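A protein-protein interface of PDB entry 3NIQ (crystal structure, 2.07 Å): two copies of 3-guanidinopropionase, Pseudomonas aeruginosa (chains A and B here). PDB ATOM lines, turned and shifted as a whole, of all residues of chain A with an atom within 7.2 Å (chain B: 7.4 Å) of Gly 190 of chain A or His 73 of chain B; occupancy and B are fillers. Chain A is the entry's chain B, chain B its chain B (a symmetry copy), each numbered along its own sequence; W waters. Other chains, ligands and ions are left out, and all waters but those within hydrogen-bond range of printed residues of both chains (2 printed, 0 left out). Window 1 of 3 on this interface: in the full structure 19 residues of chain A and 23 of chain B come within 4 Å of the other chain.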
ATOM      1  N   ALA A 149      -7.531 -34.895 -16.473  1.00  0.00           N
ATOM      2  CA  ALA A 149      -8.038 -33.566 -16.103  1.00  0.00           C
ATOM      3  C   ALA A 149      -9.507 -33.396 -16.531  1.00  0.00           C
ATOM      4  O   ALA A 149     -10.200 -32.478 -16.081  1.00  0.00           O
ATOM      5  CB  ALA A 149      -7.180 -32.457 -16.732  1.00  0.00           C
ATOM      6  N   HIS A 150      -9.966 -34.269 -17.421  1.00  0.00           N
ATOM      7  CA  HIS A 150     -11.298 -34.135 -18.011  1.00  0.00           C
ATOM      8  C   HIS A 150     -12.055 -35.454 -17.949  1.00  0.00           C
ATOM      9  O   HIS A 150     -11.463 -36.535 -18.049  1.00  0.00           O
ATOM     10  CB  HIS A 150     -11.192 -33.675 -19.476  1.00  0.00           C
ATOM     11  CG  HIS A 150     -10.156 -32.617 -19.704  1.00  0.00           C
ATOM     12  ND1 HIS A 150      -8.878 -32.909 -20.138  1.00  0.00           N
ATOM     13  CD2 HIS A 150     -10.201 -31.272 -19.533  1.00  0.00           C
ATOM     14  CE1 HIS A 150      -8.186 -31.787 -20.236  1.00  0.00           C
ATOM     15  NE2 HIS A 150      -8.963 -30.779 -19.876  1.00  0.00           N
ATOM     16  N   GLY A 187      -8.481 -36.752 -10.865  1.00  0.00           N
ATOM     17  CA  GLY A 187      -7.724 -35.585 -11.313  1.00  0.00           C
ATOM     18  C   GLY A 187      -8.513 -34.479 -11.998  1.00  0.00           C
ATOM     19  O   GLY A 187      -7.953 -33.428 -12.300  1.00  0.00           O
ATOM     20  N   ILE A 188      -9.803 -34.701 -12.237  1.00  0.00           N
ATOM     21  CA  ILE A 188     -10.653 -33.748 -12.966  1.00  0.00           C
ATOM     22  C   ILE A 188     -10.554 -32.308 -12.442  1.00  0.00           C
ATOM     23  O   ILE A 188     -10.679 -32.080 -11.239  1.00  0.00           O
ATOM     24  CB  ILE A 188     -12.152 -34.194 -12.945  1.00  0.00           C
ATOM     25  CG1 ILE A 188     -12.292 -35.720 -13.075  1.00  0.00           C
ATOM     26  CG2 ILE A 188     -12.956 -33.458 -14.000  1.00  0.00           C
ATOM     27  CD1 ILE A 188     -11.790 -36.342 -14.394  1.00  0.00           C
ATOM     28  N   ARG A 189     -10.337 -31.342 -13.344  1.00  0.00           N
ATOM     29  CA  ARG A 189     -10.152 -29.940 -12.932  1.00  0.00           C
ATOM     30  C   ARG A 189     -10.268 -28.962 -14.099  1.00  0.00           C
ATOM     31  O   ARG A 189     -10.327 -29.356 -15.263  1.00  0.00           O
ATOM     32  CB  ARG A 189      -8.776 -29.748 -12.276  1.00  0.00           C
ATOM     33  CG  ARG A 189      -7.618 -29.969 -13.246  1.00  0.00           C
ATOM     34  CD  ARG A 189      -6.270 -29.714 -12.593  1.00  0.00           C
ATOM     35  NE  ARG A 189      -5.180 -29.937 -13.548  1.00  0.00           N
ATOM     36  CZ  ARG A 189      -4.673 -31.135 -13.844  1.00  0.00           C
ATOM     37  NH1 ARG A 189      -5.155 -32.237 -13.272  1.00  0.00           N
ATOM     38  NH2 ARG A 189      -3.675 -31.234 -14.714  1.00  0.00           N
ATOM     39  N   GLY A 190     -10.250 -27.676 -13.780  1.00  0.00           N
ATOM     40  CA  GLY A 190     -10.228 -26.651 -14.816  1.00  0.00           C
ATOM     41  C   GLY A 190     -11.629 -26.201 -15.146  1.00  0.00           C
ATOM     42  O   GLY A 190     -12.596 -26.935 -14.926  1.00  0.00           O
ATOM     43  N   SER A 191     -11.720 -24.987 -15.677  1.00  0.00           N
ATOM     44  CA  SER A 191     -12.977 -24.366 -16.057  1.00  0.00           C
ATOM     45  C   SER A 191     -13.806 -25.252 -16.991  1.00  0.00           C
ATOM     46  O   SER A 191     -13.259 -26.112 -17.701  1.00  0.00           O
ATOM     47  CB  SER A 191     -12.693 -23.017 -16.722  1.00  0.00           C
ATOM     48  OG  SER A 191     -11.985 -23.201 -17.933  1.00  0.00           O
ATOM     49  N   VAL A 192     -15.124 -25.037 -16.986  1.00  0.00           N
ATOM     50  CA  VAL A 192     -16.062 -25.897 -17.709  1.00  0.00           C
ATOM     51  C   VAL A 192     -17.001 -25.084 -18.600  1.00  0.00           C
ATOM     52  O   VAL A 192     -17.206 -23.879 -18.356  1.00  0.00           O
ATOM     53  CB  VAL A 192     -16.840 -26.859 -16.748  1.00  0.00           C
ATOM     54  CG1 VAL A 192     -15.917 -27.980 -16.263  1.00  0.00           C
ATOM     55  CG2 VAL A 192     -17.399 -26.110 -15.541  1.00  0.00           C
ATOM     56  N   TYR A 193     -17.491 -25.706 -19.667  1.00  0.00           N
ATOM     57  CA  TYR A 193     -18.295 -25.026 -20.668  1.00  0.00           C
ATOM     58  C   TYR A 193     -19.611 -24.517 -20.142  1.00  0.00           C
ATOM     59  O   TYR A 193     -20.061 -23.467 -20.483  1.00  0.00           O
ATOM     60  CB  TYR A 193     -18.581 -25.930 -21.855  1.00  0.00           C
ATOM     61  CG  TYR A 193     -17.404 -26.222 -22.755  1.00  0.00           C
ATOM     62  CD1 TYR A 193     -16.657 -25.208 -23.322  1.00  0.00           C
ATOM     63  CD2 TYR A 193     -17.065 -27.524 -23.074  1.00  0.00           C
ATOM     64  CE1 TYR A 193     -15.604 -25.490 -24.142  1.00  0.00           C
ATOM     65  CE2 TYR A 193     -16.023 -27.801 -23.879  1.00  0.00           C
ATOM     66  CZ  TYR A 193     -15.293 -26.785 -24.417  1.00  0.00           C
ATOM     67  OH  TYR A 193     -14.231 -27.079 -25.215  1.00  0.00           O
ATOM     68  N   ASP A 197     -21.613 -29.729 -16.464  1.00  0.00           N
ATOM     69  CA  ASP A 197     -20.899 -30.515 -17.461  1.00  0.00           C
ATOM     70  C   ASP A 197     -21.032 -32.011 -17.155  1.00  0.00           C
ATOM     71  O   ASP A 197     -21.112 -32.842 -18.069  1.00  0.00           O
ATOM     72  CB  ASP A 197     -19.424 -30.096 -17.503  1.00  0.00           C
ATOM     73  CG  ASP A 197     -18.641 -30.815 -18.597  1.00  0.00           C
ATOM     74  OD1 ASP A 197     -19.251 -31.629 -19.336  1.00  0.00           O
ATOM     75  OD2 ASP A 197     -17.416 -30.557 -18.728  1.00  0.00           O
ATOM     76  N   HIS A 210     -12.444 -35.226  -8.408  1.00  0.00           N
ATOM     77  CA  HIS A 210     -11.815 -33.971  -8.825  1.00  0.00           C
ATOM     78  C   HIS A 210     -10.450 -33.751  -8.169  1.00  0.00           C
ATOM     79  O   HIS A 210     -10.131 -34.356  -7.136  1.00  0.00           O
ATOM     80  CB  HIS A 210     -12.742 -32.778  -8.549  1.00  0.00           C
ATOM     81  CG  HIS A 210     -13.992 -32.795  -9.372  1.00  0.00           C
ATOM     82  ND1 HIS A 210     -15.087 -33.563  -9.041  1.00  0.00           N
ATOM     83  CD2 HIS A 210     -14.312 -32.164 -10.528  1.00  0.00           C
ATOM     84  CE1 HIS A 210     -16.032 -33.396  -9.949  1.00  0.00           C
ATOM     85  NE2 HIS A 210     -15.588 -32.552 -10.863  1.00  0.00           N
ATOM     86  N   MET A 211      -9.638 -32.906  -8.796  1.00  0.00           N
ATOM     87  CA  MET A 211      -8.324 -32.566  -8.256  1.00  0.00           C
ATOM     88  C   MET A 211      -8.429 -32.107  -6.803  1.00  0.00           C
ATOM     89  O   MET A 211      -7.593 -32.484  -5.974  1.00  0.00           O
ATOM     90  CB  MET A 211      -7.639 -31.475  -9.097  1.00  0.00           C
ATOM     91  CG  MET A 211      -6.157 -31.306  -8.790  1.00  0.00           C
ATOM     92  SD  MET A 211      -5.216 -32.787  -9.172  1.00  0.00           S
ATOM     93  CE  MET A 211      -3.782 -32.478  -8.152  1.00  0.00           C
ATOM     94  N   GLU A 212      -9.440 -31.292  -6.505  1.00  0.00           N
ATOM     95  CA  GLU A 212      -9.647 -30.761  -5.129  1.00  0.00           C
ATOM     96  C   GLU A 212      -9.873 -31.897  -4.118  1.00  0.00           C
ATOM     97  O   GLU A 212      -9.201 -31.964  -3.089  1.00  0.00           O
ATOM     98  CB  GLU A 212     -10.804 -29.755  -5.084  1.00  0.00           C
ATOM     99  CG  GLU A 212     -10.572 -28.494  -5.905  1.00  0.00           C
ATOM    100  CD  GLU A 212     -10.550 -28.745  -7.414  1.00  0.00           C
ATOM    101  OE1 GLU A 212     -11.128 -29.762  -7.874  1.00  0.00           O
ATOM    102  OE2 GLU A 212      -9.958 -27.913  -8.141  1.00  0.00           O
ATOM    103  N   GLU A 256      -4.254 -28.252 -18.251  1.00  0.00           N
ATOM    104  CA  GLU A 256      -4.962 -27.497 -17.207  1.00  0.00           C
ATOM    105  C   GLU A 256      -3.974 -27.421 -16.056  1.00  0.00           C
ATOM    106  O   GLU A 256      -3.457 -28.442 -15.623  1.00  0.00           O
ATOM    107  CB  GLU A 256      -6.246 -28.212 -16.727  1.00  0.00           C
ATOM    108  CG  GLU A 256      -7.193 -28.739 -17.820  1.00  0.00           C
ATOM    109  CD  GLU A 256      -8.074 -27.651 -18.474  1.00  0.00           C
ATOM    110  OE1 GLU A 256      -8.079 -26.503 -17.998  1.00  0.00           O
ATOM    111  OE2 GLU A 256      -8.772 -27.948 -19.473  1.00  0.00           O
ATOM    112  N   ILE A 257      -3.699 -26.226 -15.550  1.00  0.00           N
ATOM    113  CA  ILE A 257      -2.711 -26.100 -14.480  1.00  0.00           C
ATOM    114  C   ILE A 257      -3.240 -26.661 -13.159  1.00  0.00           C
ATOM    115  O   ILE A 257      -4.430 -27.007 -13.038  1.00  0.00           O
ATOM    116  CB  ILE A 257      -2.254 -24.635 -14.296  1.00  0.00           C
ATOM    117  CG1 ILE A 257      -3.420 -23.763 -13.796  1.00  0.00           C
ATOM    118  CG2 ILE A 257      -1.727 -24.083 -15.644  1.00  0.00           C
ATOM    119  CD1 ILE A 257      -2.961 -22.485 -13.099  1.00  0.00           C
ATOM    120  N   ARG B  69     -12.601 -21.476 -20.186  1.00  0.00           N
ATOM    121  CA  ARG B  69     -14.019 -21.730 -20.469  1.00  0.00           C
ATOM    122  C   ARG B  69     -14.894 -20.805 -19.609  1.00  0.00           C
ATOM    123  O   ARG B  69     -14.376 -19.867 -18.990  1.00  0.00           O
ATOM    124  CB  ARG B  69     -14.338 -23.209 -20.243  1.00  0.00           C
ATOM    125  CG  ARG B  69     -13.442 -24.150 -21.065  1.00  0.00           C
ATOM    126  CD  ARG B  69     -13.697 -25.620 -20.780  1.00  0.00           C
ATOM    127  NE  ARG B  69     -12.736 -26.486 -21.466  1.00  0.00           N
ATOM    128  CZ  ARG B  69     -11.579 -26.895 -20.948  1.00  0.00           C
ATOM    129  NH1 ARG B  69     -11.212 -26.529 -19.722  1.00  0.00           N
ATOM    130  NH2 ARG B  69     -10.782 -27.680 -21.663  1.00  0.00           N
ATOM    131  N   LYS B  70     -16.203 -21.053 -19.555  1.00  0.00           N
ATOM    132  CA  LYS B  70     -17.124 -20.055 -18.980  1.00  0.00           C
ATOM    133  C   LYS B  70     -17.404 -20.144 -17.481  1.00  0.00           C
ATOM    134  O   LYS B  70     -17.822 -19.167 -16.880  1.00  0.00           O
ATOM    135  CB  LYS B  70     -18.423 -19.962 -19.791  1.00  0.00           C
ATOM    136  CG  LYS B  70     -18.179 -19.615 -21.261  1.00  0.00           C
ATOM    137  CD  LYS B  70     -19.344 -18.867 -21.908  1.00  0.00           C
ATOM    138  CE  LYS B  70     -20.459 -19.797 -22.353  1.00  0.00           C
ATOM    139  NZ  LYS B  70     -21.364 -19.097 -23.319  1.00  0.00           N
ATOM    140  N   VAL B  71     -17.160 -21.296 -16.870  1.00  0.00           N
ATOM    141  CA  VAL B  71     -17.580 -21.506 -15.485  1.00  0.00           C
ATOM    142  C   VAL B  71     -16.457 -22.060 -14.638  1.00  0.00           C
ATOM    143  O   VAL B  71     -15.756 -22.993 -15.050  1.00  0.00           O
ATOM    144  CB  VAL B  71     -18.804 -22.460 -15.387  1.00  0.00           C
ATOM    145  CG1 VAL B  71     -19.186 -22.718 -13.931  1.00  0.00           C
ATOM    146  CG2 VAL B  71     -19.983 -21.895 -16.153  1.00  0.00           C
ATOM    147  N   HIS B  72     -16.277 -21.477 -13.462  1.00  0.00           N
ATOM    148  CA  HIS B  72     -15.336 -22.018 -12.498  1.00  0.00           C
ATOM    149  C   HIS B  72     -15.891 -23.344 -11.991  1.00  0.00           C
ATOM    150  O   HIS B  72     -17.047 -23.414 -11.584  1.00  0.00           O
ATOM    151  CB  HIS B  72     -15.125 -21.038 -11.344  1.00  0.00           C
ATOM    152  CG  HIS B  72     -13.929 -21.353 -10.510  1.00  0.00           C
ATOM    153  ND1 HIS B  72     -13.871 -22.453  -9.681  1.00  0.00           N
ATOM    154  CD2 HIS B  72     -12.737 -20.723 -10.385  1.00  0.00           C
ATOM    155  CE1 HIS B  72     -12.696 -22.487  -9.079  1.00  0.00           C
ATOM    156  NE2 HIS B  72     -11.990 -21.446  -9.486  1.00  0.00           N
ATOM    157  N   HIS B  73     -15.078 -24.396 -12.013  1.00  0.00           N
ATOM    158  CA  HIS B  73     -15.589 -25.742 -11.735  1.00  0.00           C
ATOM    159  C   HIS B  73     -15.726 -26.025 -10.238  1.00  0.00           C
ATOM    160  O   HIS B  73     -16.373 -26.999  -9.846  1.00  0.00           O
ATOM    161  CB  HIS B  73     -14.705 -26.804 -12.393  1.00  0.00           C
ATOM    162  CG  HIS B  73     -13.416 -27.033 -11.670  1.00  0.00           C
ATOM    163  ND1 HIS B  73     -13.194 -28.145 -10.885  1.00  0.00           N
ATOM    164  CD2 HIS B  73     -12.294 -26.279 -11.584  1.00  0.00           C
ATOM    165  CE1 HIS B  73     -11.982 -28.077 -10.361  1.00  0.00           C
ATOM    166  NE2 HIS B  73     -11.416 -26.950 -10.764  1.00  0.00           N
ATOM    167  N   VAL B  74     -15.109 -25.189  -9.403  1.00  0.00           N
ATOM    168  CA  VAL B  74     -15.211 -25.372  -7.959  1.00  0.00           C
ATOM    169  C   VAL B  74     -16.310 -24.500  -7.371  1.00  0.00           C
ATOM    170  O   VAL B  74     -17.287 -25.006  -6.817  1.00  0.00           O
ATOM    171  CB  VAL B  74     -13.884 -25.094  -7.230  1.00  0.00           C
ATOM    172  CG1 VAL B  74     -14.038 -25.335  -5.722  1.00  0.00           C
ATOM    173  CG2 VAL B  74     -12.787 -25.975  -7.802  1.00  0.00           C
ATOM    174  N   SER B  75     -16.141 -23.192  -7.506  1.00  0.00           N
ATOM    175  CA  SER B  75     -17.098 -22.231  -6.982  1.00  0.00           C
ATOM    176  C   SER B  75     -18.357 -22.152  -7.849  1.00  0.00           C
ATOM    177  O   SER B  75     -19.355 -21.572  -7.432  1.00  0.00           O
ATOM    178  CB  SER B  75     -16.445 -20.851  -6.886  1.00  0.00           C
ATOM    179  OG  SER B  75     -16.193 -20.338  -8.185  1.00  0.00           O
ATOM    180  N   ARG B  76     -18.312 -22.711  -9.059  1.00  0.00           N
ATOM    181  CA  ARG B  76     -19.467 -22.639  -9.972  1.00  0.00           C
ATOM    182  C   ARG B  76     -19.826 -21.192 -10.374  1.00  0.00           C
ATOM    183  O   ARG B  76     -20.900 -20.946 -10.928  1.00  0.00           O
ATOM    184  CB  ARG B  76     -20.693 -23.340  -9.359  1.00  0.00           C
ATOM    185  CG  ARG B  76     -20.583 -24.853  -9.192  1.00  0.00           C
ATOM    186  CD  ARG B  76     -21.838 -25.509  -8.626  1.00  0.00           C
ATOM    187  NE  ARG B  76     -21.656 -26.947  -8.420  1.00  0.00           N
ATOM    188  CZ  ARG B  76     -22.535 -27.767  -7.834  1.00  0.00           C
ATOM    189  NH1 ARG B  76     -23.698 -27.323  -7.364  1.00  0.00           N
ATOM    190  NH2 ARG B  76     -22.240 -29.056  -7.708  1.00  0.00           N
ATOM    191  N   ILE B  77     -18.925 -20.242 -10.115  1.00  0.00           N
ATOM    192  CA  ILE B  77     -19.110 -18.852 -10.579  1.00  0.00           C
ATOM    193  C   ILE B  77     -19.060 -18.787 -12.112  1.00  0.00           C
ATOM    194  O   ILE B  77     -18.134 -19.303 -12.726  1.00  0.00           O
ATOM    195  CB  ILE B  77     -18.027 -17.896  -9.985  1.00  0.00           C
ATOM    196  CG1 ILE B  77     -18.136 -17.846  -8.456  1.00  0.00           C
ATOM    197  CG2 ILE B  77     -18.124 -16.492 -10.608  1.00  0.00           C
ATOM    198  CD1 ILE B  77     -16.883 -17.330  -7.732  1.00  0.00           C
ATOM    199  N   GLN B 266      -3.648 -21.560  -6.951  1.00  0.00           N
ATOM    200  CA  GLN B 266      -5.095 -21.626  -7.156  1.00  0.00           C
ATOM    201  C   GLN B 266      -5.889 -21.794  -5.856  1.00  0.00           C
ATOM    202  O   GLN B 266      -6.932 -21.178  -5.692  1.00  0.00           O
ATOM    203  CB  GLN B 266      -5.461 -22.746  -8.118  1.00  0.00           C
ATOM    204  CG  GLN B 266      -5.130 -22.466  -9.569  1.00  0.00           C
ATOM    205  CD  GLN B 266      -5.443 -23.657 -10.449  1.00  0.00           C
ATOM    206  OE1 GLN B 266      -4.929 -24.745 -10.226  1.00  0.00           O
ATOM    207  NE2 GLN B 266      -6.290 -23.461 -11.447  1.00  0.00           N
ATOM    208  N   ARG B 270      -8.359 -18.828  -4.580  1.00  0.00           N
ATOM    209  CA  ARG B 270      -9.736 -19.280  -4.390  1.00  0.00           C
ATOM    210  C   ARG B 270     -10.237 -19.000  -2.976  1.00  0.00           C
ATOM    211  O   ARG B 270     -11.398 -18.638  -2.796  1.00  0.00           O
ATOM    212  CB  ARG B 270      -9.858 -20.767  -4.696  1.00  0.00           C
ATOM    213  CG  ARG B 270     -10.007 -21.065  -6.171  1.00  0.00           C
ATOM    214  CD  ARG B 270      -9.699 -22.524  -6.432  1.00  0.00           C
ATOM    215  NE  ARG B 270      -9.492 -22.760  -7.856  1.00  0.00           N
ATOM    216  CZ  ARG B 270      -9.378 -23.963  -8.408  1.00  0.00           C
ATOM    217  NH1 ARG B 270      -9.456 -25.058  -7.651  1.00  0.00           N
ATOM    218  NH2 ARG B 270      -9.190 -24.069  -9.719  1.00  0.00           N
ATOM    219  N   THR B 301      -4.741 -18.364 -16.632  1.00  0.00           N
ATOM    220  CA  THR B 301      -5.548 -19.137 -15.683  1.00  0.00           C
ATOM    221  C   THR B 301      -5.695 -18.383 -14.356  1.00  0.00           C
ATOM    222  O   THR B 301      -6.794 -18.276 -13.809  1.00  0.00           O
ATOM    223  CB  THR B 301      -5.005 -20.567 -15.411  1.00  0.00           C
ATOM    224  OG1 THR B 301      -4.711 -21.234 -16.648  1.00  0.00           O
ATOM    225  CG2 THR B 301      -6.067 -21.393 -14.639  1.00  0.00           C
ATOM    226  N   PHE B 304      -8.216 -15.800 -14.846  1.00  0.00           N
ATOM    227  CA  PHE B 304      -9.574 -16.295 -14.738  1.00  0.00           C
ATOM    228  C   PHE B 304     -10.019 -16.508 -13.283  1.00  0.00           C
ATOM    229  O   PHE B 304     -11.157 -16.174 -12.940  1.00  0.00           O
ATOM    230  CB  PHE B 304      -9.788 -17.566 -15.564  1.00  0.00           C
ATOM    231  CG  PHE B 304     -11.215 -18.056 -15.550  1.00  0.00           C
ATOM    232  CD1 PHE B 304     -12.190 -17.412 -16.308  1.00  0.00           C
ATOM    233  CD2 PHE B 304     -11.585 -19.153 -14.762  1.00  0.00           C
ATOM    234  CE1 PHE B 304     -13.518 -17.841 -16.285  1.00  0.00           C
ATOM    235  CE2 PHE B 304     -12.911 -19.600 -14.742  1.00  0.00           C
ATOM    236  CZ  PHE B 304     -13.876 -18.943 -15.513  1.00  0.00           C
ATOM    237  N   GLU B 305      -9.136 -17.070 -12.453  1.00  0.00           N
ATOM    238  CA  GLU B 305      -9.419 -17.276 -11.026  1.00  0.00           C
ATOM    239  C   GLU B 305      -9.771 -15.954 -10.352  1.00  0.00           C
ATOM    240  O   GLU B 305     -10.731 -15.878  -9.584  1.00  0.00           O
ATOM    241  CB  GLU B 305      -8.211 -17.870 -10.295  1.00  0.00           C
ATOM    242  CG  GLU B 305      -7.698 -19.212 -10.828  1.00  0.00           C
ATOM    243  CD  GLU B 305      -8.549 -20.406 -10.398  1.00  0.00           C
ATOM    244  OE1 GLU B 305      -9.307 -20.283  -9.415  1.00  0.00           O
ATOM    245  OE2 GLU B 305      -8.448 -21.474 -11.044  1.00  0.00           O
ATOM    246  N   CYS B 308     -13.170 -14.341 -11.445  1.00  0.00           N
ATOM    247  CA  CYS B 308     -14.342 -14.905 -10.777  1.00  0.00           C
ATOM    248  C   CYS B 308     -14.630 -14.177  -9.465  1.00  0.00           C
ATOM    249  O   CYS B 308     -15.784 -13.851  -9.173  1.00  0.00           O
ATOM    250  CB  CYS B 308     -14.152 -16.404 -10.549  1.00  0.00           C
ATOM    251  SG  CYS B 308     -14.290 -17.314 -12.104  1.00  0.00           S
HETATM  252  O   HOH W   1      -6.884 -25.573 -13.414  1.00  0.00           O
HETATM  253  O   HOH W   2      -5.040 -23.997 -17.126  1.00  0.00           O
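NE2 of His 72 of chain B is in hydrogen-bond range of NE of Arg 270 of chain B, 3.3 Å away. The side-chain sulfur of Cys 308 of chain B sits at hydrogen-bond distance from the backbone carbonyl oxygen of Phe 304 of chain B. The side-chain carboxylate (OE1) of Glu 305 of chain B is in salt-bridge range of the guanidinium group (NE) of Arg 270 of chain B, at 2.9 Å. The guanidinium group of Arg 189 of chain A sits at hydrogen-bond distance from the backbone carbonyl oxygen of Glu 256 of chain A (2.9 Å). The guanidinium group (NH1) of Arg 189 of chain A lies within hydrogen-bond range of the backbone carbonyl oxygen (O) of Gly 187 of chain A (3.2 Å). NE2 of Gln 266 of chain B sits close to NH2 of Arg 270 of chain B, 3.4 Å away.
Water W2 lies within hydrogen-bond range of the side-chain hydroxyl (OG1) of Thr 301 of chain B (2.8 Å) and the backbone NH (N) of Ile 257 of chain A (3.0 Å). Water W1 bridges O of Ile 257 of chain A and NE2 of Gln 266 of chain B.
Of the 15 printed residues of chain B, 9 touch a printed residue of chain A. Printed residues of chain B that touch a printed residue of chain A: Arg 69, Lys 70, Val 71, His 73, Val 74, Gln 266, Arg 270, Thr 301 and Phe 304. Hydrophobic or aromatic side chains of chain A within 4 Å of the printed part of chain B: Val 192, Tyr 193 and Ile 257. Among the printed residues, Asp or Glu carboxylates within 4 Å of a Lys or Arg side-chain nitrogen of the other chain: Glu 212 of chain A with Arg 270 of chain B (2.9 Å) and Glu 256 of chain A with Arg 69 of chain B (2.8 Å).
Ala 149 of chain A touches none of the printed residues of chain B. Gly 190 of chain A touches just one residue of chain B: His 73 (3.3 Å). Of the printed residues of chain B, Ser 191 of chain A touches Arg 69, Val 71 and Phe 304. Of the printed residues of chain A, Arg 69 of chain B touches Ser 191, Val 192, Tyr 193 and Glu 256. Of chain A, only Arg 189, Gly 190 and Glu 212 come within 4 Å of His 73 of chain B. Of the printed residues of chain A, Val 74 of chain B touches Glu 212 (3.4 Å). Of the printed residues of chain A, Arg 270 of chain B touches Glu 212. Of the printed residues of chain A, Thr 301 of chain B touches Ile 257 (3.6 Å). The nearest printed residue of chain A that does not touch His 73 of chain B is His 210 of chain A (4.2 Å). The nearest printed residue of chain B that does not touch Glu 256 of chain A is Thr 301 of chain B (6.3 Å).
Among the printed residues, pairs that only touch across the chains: Ser 191 of chain A with Val 71 of chain B (3.3 Å), Glu 212 of chain A with Val 74 of chain B (3.4 Å), Val 192 of chain A with Arg 69 of chain B (3.5 Å), Ile 257 of chain A with Thr 301 of chain B (3.6 Å), Ile 257 of chain A with Gln 266 of chain B (3.6 Å), Arg 189 of chain A with His 73 of chain B (3.7 Å), Tyr 193 of chain A with Arg 69 of chain B (3.9 Å), Tyr 193 of chain A with Lys 70 of chain B (3.9 Å) and Ser 191 of chain A with Phe 304 of chain B (3.96 Å).
A ring nitrogen (NE2) of His 73 of chain B sits close to the side-chain carboxylate of Glu 212 of chain A, 3.2 Å away. N of Arg 69 of chain B lies within hydrogen-bond range of OG of Ser 191 of chain A (2.9 Å). The backbone NH of Val 192 of chain A is in hydrogen-bond range of the backbone carbonyl oxygen of Val 71 of chain B (2.9 Å). N of Gly 190 of chain A sits close to NE2 of His 73 of chain B. The side-chain carboxylate (OE2) of Glu 256 of chain A lies within salt-bridge range of the guanidinium group (NH1) of Arg 69 of chain B, at 2.8 Å. NH1 of Arg 270 of chain B lies within salt-bridge range of OE2 of Glu 212 of chain A (2.9 Å). The backbone carbonyl oxygen (O) of Val 192 of chain A is in hydrogen-bond range of the backbone NH (N) of Lys 70 of chain B, 3.2 Å away.
No position is printed for both chains.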
